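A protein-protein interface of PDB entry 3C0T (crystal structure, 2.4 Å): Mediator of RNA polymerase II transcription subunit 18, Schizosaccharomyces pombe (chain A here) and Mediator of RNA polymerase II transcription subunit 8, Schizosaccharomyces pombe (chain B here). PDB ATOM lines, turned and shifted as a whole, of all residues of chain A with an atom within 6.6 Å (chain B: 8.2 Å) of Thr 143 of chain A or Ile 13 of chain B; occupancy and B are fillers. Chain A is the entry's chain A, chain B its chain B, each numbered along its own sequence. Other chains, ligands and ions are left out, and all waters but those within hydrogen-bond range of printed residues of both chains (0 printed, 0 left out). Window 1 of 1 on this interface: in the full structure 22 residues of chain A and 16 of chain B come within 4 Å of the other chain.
ND2 of Asn 160 of chain A is in hydrogen-bond range of O of Ala 25 of chain B (2.8 Å). The backbone carbonyl oxygen of Met 159 of chain A sits close to the backbone carbonyl oxygen of Leu 26 of chain B (3.5 Å).
The side-chain amide oxygen of Gln 163 of chain A is in hydrogen-bond range of the backbone NH of Met 159 of chain A, at 2.7 Å. The side-chain amide nitrogen of Gln 142 of chain A lies within hydrogen-bond range of the backbone carbonyl oxygen of Gln 163 of chain A, at 3.3 Å. O of Tyr 141 of chain A lies within hydrogen-bond range of N of Ile 166 of chain A (2.7 Å). N of Ile 145 of chain A is in hydrogen-bond range of O of His 157 of chain A, at 2.7 Å. NE of Arg 22 of chain B lies within hydrogen-bond range of O of Leu 26 of chain B (3.1 Å). The side-chain sulfur (SD) of Met 159 of chain A sits at hydrogen-bond distance from the side-chain hydroxyl (OG1) of Thr 143 of chain A (3.6 Å).
OH of Tyr 141 of chain A touches CE of Met 17 of chain B (3.5 Å). Thr 143 of chain A touches Ile 13 of chain B (CG2 to CG2, 3.4 Å). Arg 22 of chain B touches Ile 145 of chain A (NH2 to CG1, 3.8 Å). Met 159 of chain A touches Phe 16 of chain B (CE to CD2, 3.3 Å). Met 159 of chain A touches Arg 22 of chain B. Gln 163 of chain A touches Met 9 of chain B. Ile 13 of chain B touches Gln 163 of chain A (CD1 to CG, 3.8 Å). CD of Pro 164 of chain A touches CB of Met 9 of chain B (3.7 Å). Ile 166 of chain A touches Leu 10 of chain B (CD1 to CD1, 3.8 Å). CD1 of Ile 166 of chain A touches CG2 of Ile 13 of chain B (3.9 Å).
Thr 143 of chain A touches just these residues of chain B: Ile 13 and Met 17. Of chain A, only Thr 143 (3.4 Å), Gln 163 (3.8 Å) and Ile 166 (3.9 Å) come within 4 Å of Ile 13 of chain B. Of the printed residues of chain B, Tyr 124 of chain A touches Phe 16 (3.8 Å) and Met 17 (3.7 Å). Of the printed residues of chain B, Gln 163 of chain A touches Met 9 and Ile 13. Of the printed residues of chain A, Met 17 of chain B touches Tyr 124 (3.7 Å), Tyr 141 (3.5 Å) and Thr 143 (3.5 Å). The nearest residue of chain A that does not touch Ile 13 of chain B is Pro 164 of chain A (4.5 Å). The nearest printed residue of chain B that does not touch Ile 145 of chain A is Leu 26 of chain B (7.2 Å).
Printed residues of chain A that touch a printed residue of chain B: Tyr 124, Tyr 141, Thr 143, Ile 145, Met 159, Asn 160, Gln 163, Pro 164 and Ile 166. Printed residues of chain B that touch a printed residue of chain A: Met 9, Leu 10, Ile 13, Phe 16, Met 17, Arg 22, Ala 25 and Leu 26. Hydrophobic or aromatic side chains of chain B that line the printed part of chain A: Met 9, Leu 10, Ile 13, Phe 16, Met 17 and Leu 26. Along chain B the printed residues that touch a printed residue of chain A span positions 9 to 26. Among the printed residues, 17 pairs touch across the chains. Among the printed residues, no Asp or Glu carboxylate lies within 4 Å of a Lys or Arg side-chain nitrogen of the other chain.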
ATOM      1  N   TYR A 124     -26.338  24.881  25.189  1.00  0.00           N
ATOM      2  CA  TYR A 124     -25.164  25.561  24.670  1.00  0.00           C
ATOM      3  C   TYR A 124     -24.445  24.668  23.678  1.00  0.00           C
ATOM      4  O   TYR A 124     -24.794  23.496  23.491  1.00  0.00           O
ATOM      5  CB  TYR A 124     -24.199  25.977  25.801  1.00  0.00           C
ATOM      6  CG  TYR A 124     -23.815  24.859  26.737  1.00  0.00           C
ATOM      7  CD1 TYR A 124     -24.636  24.512  27.804  1.00  0.00           C
ATOM      8  CD2 TYR A 124     -22.644  24.119  26.531  1.00  0.00           C
ATOM      9  CE1 TYR A 124     -24.311  23.455  28.646  1.00  0.00           C
ATOM     10  CE2 TYR A 124     -22.303  23.061  27.369  1.00  0.00           C
ATOM     11  CZ  TYR A 124     -23.144  22.733  28.427  1.00  0.00           C
ATOM     12  OH  TYR A 124     -22.819  21.695  29.272  1.00  0.00           O
ATOM     13  N   ILE A 125     -23.440  25.241  23.038  1.00  0.00           N
ATOM     14  CA  ILE A 125     -22.664  24.537  22.041  1.00  0.00           C
ATOM     15  C   ILE A 125     -21.194  24.520  22.445  1.00  0.00           C
ATOM     16  O   ILE A 125     -20.682  25.500  22.986  1.00  0.00           O
ATOM     17  CB  ILE A 125     -22.831  25.226  20.668  1.00  0.00           C
ATOM     18  CG1 ILE A 125     -24.226  24.916  20.116  1.00  0.00           C
ATOM     19  CG2 ILE A 125     -21.726  24.786  19.706  1.00  0.00           C
ATOM     20  CD1 ILE A 125     -24.565  25.653  18.832  1.00  0.00           C
ATOM     21  N   ILE A 126     -20.532  23.389  22.218  1.00  0.00           N
ATOM     22  CA  ILE A 126     -19.114  23.268  22.533  1.00  0.00           C
ATOM     23  C   ILE A 126     -18.342  23.162  21.224  1.00  0.00           C
ATOM     24  O   ILE A 126     -18.625  22.304  20.374  1.00  0.00           O
ATOM     25  CB  ILE A 126     -18.780  22.019  23.391  1.00  0.00           C
ATOM     26  CG1 ILE A 126     -19.427  22.125  24.779  1.00  0.00           C
ATOM     27  CG2 ILE A 126     -17.265  21.903  23.559  1.00  0.00           C
ATOM     28  CD1 ILE A 126     -19.059  23.389  25.541  1.00  0.00           C
ATOM     29  N   GLN A 127     -17.371  24.057  21.083  1.00  0.00           N
ATOM     30  CA  GLN A 127     -16.507  24.133  19.922  1.00  0.00           C
ATOM     31  C   GLN A 127     -15.074  23.930  20.408  1.00  0.00           C
ATOM     32  O   GLN A 127     -14.632  24.626  21.329  1.00  0.00           O
ATOM     33  CB  GLN A 127     -16.623  25.525  19.296  1.00  0.00           C
ATOM     34  CG  GLN A 127     -15.575  25.837  18.232  1.00  0.00           C
ATOM     35  CD  GLN A 127     -15.398  27.340  18.010  1.00  0.00           C
ATOM     36  OE1 GLN A 127     -15.340  27.801  16.877  1.00  0.00           O
ATOM     37  NE2 GLN A 127     -15.306  28.101  19.094  1.00  0.00           N
ATOM     38  N   TYR A 141     -11.530  23.934  24.426  1.00  0.00           N
ATOM     39  CA  TYR A 141     -12.786  24.364  23.825  1.00  0.00           C
ATOM     40  C   TYR A 141     -13.327  25.704  24.270  1.00  0.00           C
ATOM     41  O   TYR A 141     -12.835  26.329  25.205  1.00  0.00           O
ATOM     42  CB  TYR A 141     -13.871  23.322  24.111  1.00  0.00           C
ATOM     43  CG  TYR A 141     -14.280  23.263  25.572  1.00  0.00           C
ATOM     44  CD1 TYR A 141     -13.535  22.536  26.505  1.00  0.00           C
ATOM     45  CD2 TYR A 141     -15.414  23.939  26.028  1.00  0.00           C
ATOM     46  CE1 TYR A 141     -13.907  22.481  27.848  1.00  0.00           C
ATOM     47  CE2 TYR A 141     -15.795  23.894  27.374  1.00  0.00           C
ATOM     48  CZ  TYR A 141     -15.038  23.163  28.278  1.00  0.00           C
ATOM     49  OH  TYR A 141     -15.417  23.106  29.612  1.00  0.00           O
ATOM     50  N   GLN A 142     -14.392  26.110  23.592  1.00  0.00           N
ATOM     51  CA  GLN A 142     -15.068  27.358  23.875  1.00  0.00           C
ATOM     52  C   GLN A 142     -16.547  27.015  23.957  1.00  0.00           C
ATOM     53  O   GLN A 142     -17.029  26.173  23.195  1.00  0.00           O
ATOM     54  CB  GLN A 142     -14.810  28.337  22.734  1.00  0.00           C
ATOM     55  CG  GLN A 142     -14.847  29.787  23.159  1.00  0.00           C
ATOM     56  CD  GLN A 142     -14.112  30.670  22.189  1.00  0.00           C
ATOM     57  OE1 GLN A 142     -14.511  30.805  21.022  1.00  0.00           O
ATOM     58  NE2 GLN A 142     -13.015  31.267  22.653  1.00  0.00           N
ATOM     59  N   THR A 143     -17.276  27.619  24.889  1.00  0.00           N
ATOM     60  CA  THR A 143     -18.693  27.310  24.954  1.00  0.00           C
ATOM     61  C   THR A 143     -19.464  28.452  24.295  1.00  0.00           C
ATOM     62  O   THR A 143     -19.307  29.629  24.640  1.00  0.00           O
ATOM     63  CB  THR A 143     -19.165  27.001  26.413  1.00  0.00           C
ATOM     64  OG1 THR A 143     -19.926  28.086  26.932  1.00  0.00           O
ATOM     65  CG2 THR A 143     -17.990  26.720  27.301  1.00  0.00           C
ATOM     66  N   LEU A 144     -20.257  28.079  23.296  1.00  0.00           N
ATOM     67  CA  LEU A 144     -21.031  29.021  22.506  1.00  0.00           C
ATOM     68  C   LEU A 144     -22.530  28.989  22.760  1.00  0.00           C
ATOM     69  O   LEU A 144     -23.035  28.117  23.462  1.00  0.00           O
ATOM     70  CB  LEU A 144     -20.745  28.767  21.024  1.00  0.00           C
ATOM     71  CG  LEU A 144     -19.474  29.357  20.384  1.00  0.00           C
ATOM     72  CD1 LEU A 144     -18.512  29.911  21.429  1.00  0.00           C
ATOM     73  CD2 LEU A 144     -18.808  28.284  19.532  1.00  0.00           C
ATOM     74  N   ILE A 145     -23.232  29.948  22.165  1.00  0.00           N
ATOM     75  CA  ILE A 145     -24.678  30.079  22.303  1.00  0.00           C
ATOM     76  C   ILE A 145     -25.318  30.100  20.921  1.00  0.00           C
ATOM     77  O   ILE A 145     -24.913  30.877  20.061  1.00  0.00           O
ATOM     78  CB  ILE A 145     -25.043  31.413  23.031  1.00  0.00           C
ATOM     79  CG1 ILE A 145     -24.356  31.472  24.397  1.00  0.00           C
ATOM     80  CG2 ILE A 145     -26.551  31.531  23.205  1.00  0.00           C
ATOM     81  CD1 ILE A 145     -24.733  30.326  25.306  1.00  0.00           C
ATOM     82  N   HIS A 157     -22.683  32.213  18.959  1.00  0.00           N
ATOM     83  CA  HIS A 157     -22.024  33.335  19.611  1.00  0.00           C
ATOM     84  C   HIS A 157     -21.344  33.004  20.921  1.00  0.00           C
ATOM     85  O   HIS A 157     -21.846  32.209  21.714  1.00  0.00           O
ATOM     86  CB  HIS A 157     -23.027  34.463  19.881  1.00  0.00           C
ATOM     87  CG  HIS A 157     -23.796  34.892  18.674  1.00  0.00           C
ATOM     88  ND1 HIS A 157     -25.136  34.617  18.512  1.00  0.00           N
ATOM     89  CD2 HIS A 157     -23.406  35.549  17.556  1.00  0.00           C
ATOM     90  CE1 HIS A 157     -25.539  35.085  17.343  1.00  0.00           C
ATOM     91  NE2 HIS A 157     -24.508  35.654  16.744  1.00  0.00           N
ATOM     92  N   PRO A 158     -20.176  33.613  21.168  1.00  0.00           N
ATOM     93  CA  PRO A 158     -19.495  33.334  22.435  1.00  0.00           C
ATOM     94  C   PRO A 158     -20.316  34.053  23.508  1.00  0.00           C
ATOM     95  O   PRO A 158     -21.103  34.945  23.191  1.00  0.00           O
ATOM     96  CB  PRO A 158     -18.114  33.958  22.231  1.00  0.00           C
ATOM     97  CG  PRO A 158     -18.408  35.125  21.320  1.00  0.00           C
ATOM     98  CD  PRO A 158     -19.374  34.515  20.319  1.00  0.00           C
ATOM     99  N   MET A 159     -20.155  33.666  24.764  1.00  0.00           N
ATOM    100  CA  MET A 159     -20.906  34.314  25.828  1.00  0.00           C
ATOM    101  C   MET A 159     -20.288  35.670  26.155  1.00  0.00           C
ATOM    102  O   MET A 159     -20.915  36.516  26.790  1.00  0.00           O
ATOM    103  CB  MET A 159     -20.918  33.424  27.063  1.00  0.00           C
ATOM    104  CG  MET A 159     -21.420  32.027  26.774  1.00  0.00           C
ATOM    105  SD  MET A 159     -21.521  31.048  28.258  1.00  0.00           S
ATOM    106  CE  MET A 159     -22.973  31.811  28.990  1.00  0.00           C
ATOM    107  N   ASN A 160     -19.053  35.865  25.704  1.00  0.00           N
ATOM    108  CA  ASN A 160     -18.316  37.101  25.926  1.00  0.00           C
ATOM    109  C   ASN A 160     -17.323  37.260  24.784  1.00  0.00           C
ATOM    110  O   ASN A 160     -16.827  36.270  24.253  1.00  0.00           O
ATOM    111  CB  ASN A 160     -17.578  37.033  27.260  1.00  0.00           C
ATOM    112  CG  ASN A 160     -16.933  38.352  27.635  1.00  0.00           C
ATOM    113  OD1 ASN A 160     -16.033  38.840  26.947  1.00  0.00           O
ATOM    114  ND2 ASN A 160     -17.397  38.944  28.733  1.00  0.00           N
ATOM    115  N   GLN A 163     -13.624  35.939  25.537  1.00  0.00           N
ATOM    116  CA  GLN A 163     -13.751  34.611  26.112  1.00  0.00           C
ATOM    117  C   GLN A 163     -12.515  33.738  25.950  1.00  0.00           C
ATOM    118  O   GLN A 163     -12.035  33.531  24.838  1.00  0.00           O
ATOM    119  CB  GLN A 163     -14.937  33.917  25.457  1.00  0.00           C
ATOM    120  CG  GLN A 163     -15.424  32.699  26.178  1.00  0.00           C
ATOM    121  CD  GLN A 163     -16.701  32.183  25.569  1.00  0.00           C
ATOM    122  OE1 GLN A 163     -17.671  32.920  25.445  1.00  0.00           O
ATOM    123  NE2 GLN A 163     -16.709  30.914  25.180  1.00  0.00           N
ATOM    124  N   PRO A 164     -11.977  33.220  27.062  1.00  0.00           N
ATOM    125  CA  PRO A 164     -10.793  32.363  26.962  1.00  0.00           C
ATOM    126  C   PRO A 164     -11.222  30.953  26.544  1.00  0.00           C
ATOM    127  O   PRO A 164     -12.409  30.608  26.618  1.00  0.00           O
ATOM    128  CB  PRO A 164     -10.246  32.375  28.382  1.00  0.00           C
ATOM    129  CG  PRO A 164     -11.509  32.411  29.197  1.00  0.00           C
ATOM    130  CD  PRO A 164     -12.328  33.459  28.472  1.00  0.00           C
ATOM    131  N   ILE A 166     -11.120  26.932  27.177  1.00  0.00           N
ATOM    132  CA  ILE A 166     -10.982  26.107  28.367  1.00  0.00           C
ATOM    133  C   ILE A 166     -10.195  24.858  28.012  1.00  0.00           C
ATOM    134  O   ILE A 166     -10.445  24.232  26.977  1.00  0.00           O
ATOM    135  CB  ILE A 166     -12.366  25.708  28.932  1.00  0.00           C
ATOM    136  CG1 ILE A 166     -13.091  26.954  29.443  1.00  0.00           C
ATOM    137  CG2 ILE A 166     -12.212  24.679  30.062  1.00  0.00           C
ATOM    138  CD1 ILE A 166     -14.480  26.682  29.969  1.00  0.00           C
ATOM    139  N   ALA B   6      -9.162  35.847  33.416  1.00  0.00           N
ATOM    140  CA  ALA B   6      -9.488  34.668  32.616  1.00  0.00           C
ATOM    141  C   ALA B   6      -9.926  33.542  33.553  1.00  0.00           C
ATOM    142  O   ALA B   6     -10.660  32.638  33.156  1.00  0.00           O
ATOM    143  CB  ALA B   6      -8.282  34.235  31.798  1.00  0.00           C
ATOM    144  N   ASN B   7      -9.469  33.606  34.801  1.00  0.00           N
ATOM    145  CA  ASN B   7      -9.827  32.609  35.799  1.00  0.00           C
ATOM    146  C   ASN B   7     -11.225  32.869  36.344  1.00  0.00           C
ATOM    147  O   ASN B   7     -11.880  31.963  36.861  1.00  0.00           O
ATOM    148  CB  ASN B   7      -8.798  32.607  36.929  1.00  0.00           C
ATOM    149  CG  ASN B   7      -7.572  31.780  36.587  1.00  0.00           C
ATOM    150  OD1 ASN B   7      -7.619  30.544  36.600  1.00  0.00           O
ATOM    151  ND2 ASN B   7      -6.470  32.452  36.263  1.00  0.00           N
ATOM    152  N   GLN B   8     -11.679  34.111  36.228  1.00  0.00           N
ATOM    153  CA  GLN B   8     -13.019  34.462  36.676  1.00  0.00           C
ATOM    154  C   GLN B   8     -13.985  34.027  35.568  1.00  0.00           C
ATOM    155  O   GLN B   8     -15.096  33.573  35.840  1.00  0.00           O
ATOM    156  CB  GLN B   8     -13.133  35.970  36.922  1.00  0.00           C
ATOM    157  CG  GLN B   8     -14.540  36.426  37.298  1.00  0.00           C
ATOM    158  CD  GLN B   8     -15.074  35.738  38.548  1.00  0.00           C
ATOM    159  OE1 GLN B   8     -16.277  35.759  38.816  1.00  0.00           O
ATOM    160  NE2 GLN B   8     -14.179  35.129  39.322  1.00  0.00           N
ATOM    161  N   MET B   9     -13.550  34.170  34.319  1.00  0.00           N
ATOM    162  CA  MET B   9     -14.353  33.758  33.177  1.00  0.00           C
ATOM    163  C   MET B   9     -14.612  32.270  33.302  1.00  0.00           C
ATOM    164  O   MET B   9     -15.740  31.808  33.154  1.00  0.00           O
ATOM    165  CB  MET B   9     -13.605  34.023  31.870  1.00  0.00           C
ATOM    166  CG  MET B   9     -13.560  35.472  31.473  1.00  0.00           C
ATOM    167  SD  MET B   9     -15.198  36.025  31.009  1.00  0.00           S
ATOM    168  CE  MET B   9     -14.983  36.208  29.252  1.00  0.00           C
ATOM    169  N   LEU B  10     -13.545  31.527  33.581  1.00  0.00           N
ATOM    170  CA  LEU B  10     -13.618  30.085  33.732  1.00  0.00           C
ATOM    171  C   LEU B  10     -14.694  29.699  34.729  1.00  0.00           C
ATOM    172  O   LEU B  10     -15.505  28.812  34.468  1.00  0.00           O
ATOM    173  CB  LEU B  10     -12.281  29.526  34.214  1.00  0.00           C
ATOM    174  CG  LEU B  10     -12.293  28.020  34.482  1.00  0.00           C
ATOM    175  CD1 LEU B  10     -12.572  27.259  33.192  1.00  0.00           C
ATOM    176  CD2 LEU B  10     -10.959  27.606  35.064  1.00  0.00           C
ATOM    177  N   THR B  11     -14.697  30.369  35.874  1.00  0.00           N
ATOM    178  CA  THR B  11     -15.675  30.074  36.904  1.00  0.00           C
ATOM    179  C   THR B  11     -17.095  30.383  36.456  1.00  0.00           C
ATOM    180  O   THR B  11     -18.007  29.589  36.688  1.00  0.00           O
ATOM    181  CB  THR B  11     -15.347  30.846  38.198  1.00  0.00           C
ATOM    182  OG1 THR B  11     -14.105  30.362  38.723  1.00  0.00           O
ATOM    183  CG2 THR B  11     -16.436  30.651  39.245  1.00  0.00           C
ATOM    184  N   ASP B  12     -17.289  31.522  35.806  1.00  0.00           N
ATOM    185  CA  ASP B  12     -18.622  31.886  35.344  1.00  0.00           C
ATOM    186  C   ASP B  12     -19.105  30.967  34.221  1.00  0.00           C
ATOM    187  O   ASP B  12     -20.276  30.595  34.187  1.00  0.00           O
ATOM    188  CB  ASP B  12     -18.657  33.340  34.860  1.00  0.00           C
ATOM    189  CG  ASP B  12     -18.330  34.342  35.965  1.00  0.00           C
ATOM    190  OD1 ASP B  12     -18.546  34.020  37.159  1.00  0.00           O
ATOM    191  OD2 ASP B  12     -17.861  35.457  35.626  1.00  0.00           O
ATOM    192  N   ILE B  13     -18.207  30.608  33.302  1.00  0.00           N
ATOM    193  CA  ILE B  13     -18.572  29.735  32.192  1.00  0.00           C
ATOM    194  C   ILE B  13     -18.915  28.354  32.729  1.00  0.00           C
ATOM    195  O   ILE B  13     -19.917  27.762  32.325  1.00  0.00           O
ATOM    196  CB  ILE B  13     -17.438  29.636  31.150  1.00  0.00           C
ATOM    197  CG1 ILE B  13     -17.197  31.020  30.527  1.00  0.00           C
ATOM    198  CG2 ILE B  13     -17.810  28.638  30.053  1.00  0.00           C
ATOM    199  CD1 ILE B  13     -15.976  31.088  29.603  1.00  0.00           C
ATOM    200  N   LEU B  14     -18.101  27.847  33.649  1.00  0.00           N
ATOM    201  CA  LEU B  14     -18.366  26.543  34.234  1.00  0.00           C
ATOM    202  C   LEU B  14     -19.711  26.550  34.963  1.00  0.00           C
ATOM    203  O   LEU B  14     -20.451  25.562  34.920  1.00  0.00           O
ATOM    204  CB  LEU B  14     -17.250  26.151  35.202  1.00  0.00           C
ATOM    205  CG  LEU B  14     -15.901  25.820  34.560  1.00  0.00           C
ATOM    206  CD1 LEU B  14     -14.889  25.416  35.637  1.00  0.00           C
ATOM    207  CD2 LEU B  14     -16.079  24.691  33.557  1.00  0.00           C
ATOM    208  N   SER B  15     -20.029  27.664  35.624  1.00  0.00           N
ATOM    209  CA  SER B  15     -21.293  27.796  36.357  1.00  0.00           C
ATOM    210  C   SER B  15     -22.472  27.782  35.407  1.00  0.00           C
ATOM    211  O   SER B  15     -23.497  27.172  35.697  1.00  0.00           O
ATOM    212  CB  SER B  15     -21.337  29.100  37.166  1.00  0.00           C
ATOM    213  OG  SER B  15     -20.440  29.055  38.260  1.00  0.00           O
ATOM    214  N   PHE B  16     -22.341  28.475  34.281  1.00  0.00           N
ATOM    215  CA  PHE B  16     -23.418  28.507  33.304  1.00  0.00           C
ATOM    216  C   PHE B  16     -23.726  27.107  32.786  1.00  0.00           C
ATOM    217  O   PHE B  16     -24.886  26.693  32.734  1.00  0.00           O
ATOM    218  CB  PHE B  16     -23.052  29.379  32.110  1.00  0.00           C
ATOM    219  CG  PHE B  16     -23.997  29.218  30.958  1.00  0.00           C
ATOM    220  CD1 PHE B  16     -25.338  29.586  31.086  1.00  0.00           C
ATOM    221  CD2 PHE B  16     -23.574  28.640  29.767  1.00  0.00           C
ATOM    222  CE1 PHE B  16     -26.246  29.376  30.045  1.00  0.00           C
ATOM    223  CE2 PHE B  16     -24.475  28.426  28.719  1.00  0.00           C
ATOM    224  CZ  PHE B  16     -25.814  28.796  28.862  1.00  0.00           C
ATOM    225  N   MET B  17     -22.686  26.382  32.386  1.00  0.00           N
ATOM    226  CA  MET B  17     -22.877  25.041  31.871  1.00  0.00           C
ATOM    227  C   MET B  17     -23.503  24.153  32.937  1.00  0.00           C
ATOM    228  O   MET B  17     -24.379  23.340  32.639  1.00  0.00           O
ATOM    229  CB  MET B  17     -21.541  24.460  31.409  1.00  0.00           C
ATOM    230  CG  MET B  17     -20.895  25.281  30.296  1.00  0.00           C
ATOM    231  SD  MET B  17     -19.471  24.487  29.537  1.00  0.00           S
ATOM    232  CE  MET B  17     -18.277  24.603  30.860  1.00  0.00           C
ATOM    233  N   LYS B  18     -23.076  24.326  34.185  1.00  0.00           N
ATOM    234  CA  LYS B  18     -23.601  23.505  35.258  1.00  0.00           C
ATOM    235  C   LYS B  18     -25.034  23.834  35.658  1.00  0.00           C
ATOM    236  O   LYS B  18     -25.872  22.934  35.740  1.00  0.00           O
ATOM    237  CB  LYS B  18     -22.708  23.592  36.500  1.00  0.00           C
ATOM    238  CG  LYS B  18     -23.067  22.560  37.575  1.00  0.00           C
ATOM    239  CD  LYS B  18     -22.143  22.657  38.775  1.00  0.00           C
ATOM    240  CE  LYS B  18     -22.521  21.672  39.870  1.00  0.00           C
ATOM    241  NZ  LYS B  18     -22.281  20.263  39.472  1.00  0.00           N
ATOM    242  N   SER B  19     -25.328  25.114  35.880  1.00  0.00           N
ATOM    243  CA  SER B  19     -26.666  25.495  36.325  1.00  0.00           C
ATOM    244  C   SER B  19     -27.457  26.464  35.462  1.00  0.00           C
ATOM    245  O   SER B  19     -28.558  26.855  35.837  1.00  0.00           O
ATOM    246  CB  SER B  19     -26.591  26.065  37.743  1.00  0.00           C
ATOM    247  OG  SER B  19     -25.907  27.308  37.756  1.00  0.00           O
ATOM    248  N   GLY B  20     -26.922  26.854  34.315  1.00  0.00           N
ATOM    249  CA  GLY B  20     -27.650  27.781  33.469  1.00  0.00           C
ATOM    250  C   GLY B  20     -27.610  29.212  33.984  1.00  0.00           C
ATOM    251  O   GLY B  20     -28.189  30.111  33.371  1.00  0.00           O
ATOM    252  N   LYS B  21     -26.939  29.426  35.113  1.00  0.00           N
ATOM    253  CA  LYS B  21     -26.811  30.765  35.685  1.00  0.00           C
ATOM    254  C   LYS B  21     -25.846  31.571  34.835  1.00  0.00           C
ATOM    255  O   LYS B  21     -24.685  31.195  34.658  1.00  0.00           O
ATOM    256  CB  LYS B  21     -26.281  30.707  37.122  1.00  0.00           C
ATOM    257  CG  LYS B  21     -27.295  30.242  38.155  1.00  0.00           C
ATOM    258  CD  LYS B  21     -26.653  30.127  39.530  1.00  0.00           C
ATOM    259  CE  LYS B  21     -27.654  29.663  40.574  1.00  0.00           C
ATOM    260  NZ  LYS B  21     -27.001  29.429  41.898  1.00  0.00           N
ATOM    261  N   ARG B  22     -26.328  32.690  34.316  1.00  0.00           N
ATOM    262  CA  ARG B  22     -25.507  33.537  33.470  1.00  0.00           C
ATOM    263  C   ARG B  22     -25.035  34.762  34.247  1.00  0.00           C
ATOM    264  O   ARG B  22     -25.817  35.669  34.521  1.00  0.00           O
ATOM    265  CB  ARG B  22     -26.318  33.946  32.240  1.00  0.00           C
ATOM    266  CG  ARG B  22     -25.487  34.318  31.037  1.00  0.00           C
ATOM    267  CD  ARG B  22     -26.258  34.056  29.755  1.00  0.00           C
ATOM    268  NE  ARG B  22     -25.502  34.476  28.579  1.00  0.00           N
ATOM    269  CZ  ARG B  22     -25.865  34.220  27.326  1.00  0.00           C
ATOM    270  NH1 ARG B  22     -26.978  33.536  27.083  1.00  0.00           N
ATOM    271  NH2 ARG B  22     -25.120  34.656  26.318  1.00  0.00           N
ATOM    272  N   ALA B  23     -23.754  34.771  34.612  1.00  0.00           N
ATOM    273  CA  ALA B  23     -23.166  35.884  35.358  1.00  0.00           C
ATOM    274  C   ALA B  23     -23.238  37.170  34.542  1.00  0.00           C
ATOM    275  O   ALA B  23     -23.338  37.129  33.316  1.00  0.00           O
ATOM    276  CB  ALA B  23     -21.717  35.573  35.709  1.00  0.00           C
ATOM    277  N   ALA B  25     -20.962  39.225  33.830  1.00  0.00           N
ATOM    278  CA  ALA B  25     -19.809  39.279  32.932  1.00  0.00           C
ATOM    279  C   ALA B  25     -20.071  38.563  31.607  1.00  0.00           C
ATOM    280  O   ALA B  25     -19.474  38.895  30.583  1.00  0.00           O
ATOM    281  CB  ALA B  25     -18.592  38.671  33.619  1.00  0.00           C
ATOM    282  N   LEU B  26     -20.960  37.574  31.633  1.00  0.00           N
ATOM    283  CA  LEU B  26     -21.308  36.812  30.439  1.00  0.00           C
ATOM    284  C   LEU B  26     -22.562  37.402  29.799  1.00  0.00           C
ATOM    285  O   LEU B  26     -23.376  36.683  29.214  1.00  0.00           O
ATOM    286  CB  LEU B  26     -21.542  35.344  30.806  1.00  0.00           C
ATOM    287  CG  LEU B  26     -20.359  34.652  31.494  1.00  0.00           C
ATOM    288  CD1 LEU B  26     -20.751  33.249  31.910  1.00  0.00           C
ATOM    289  CD2 LEU B  26     -19.161  34.624  30.554  1.00  0.00           C
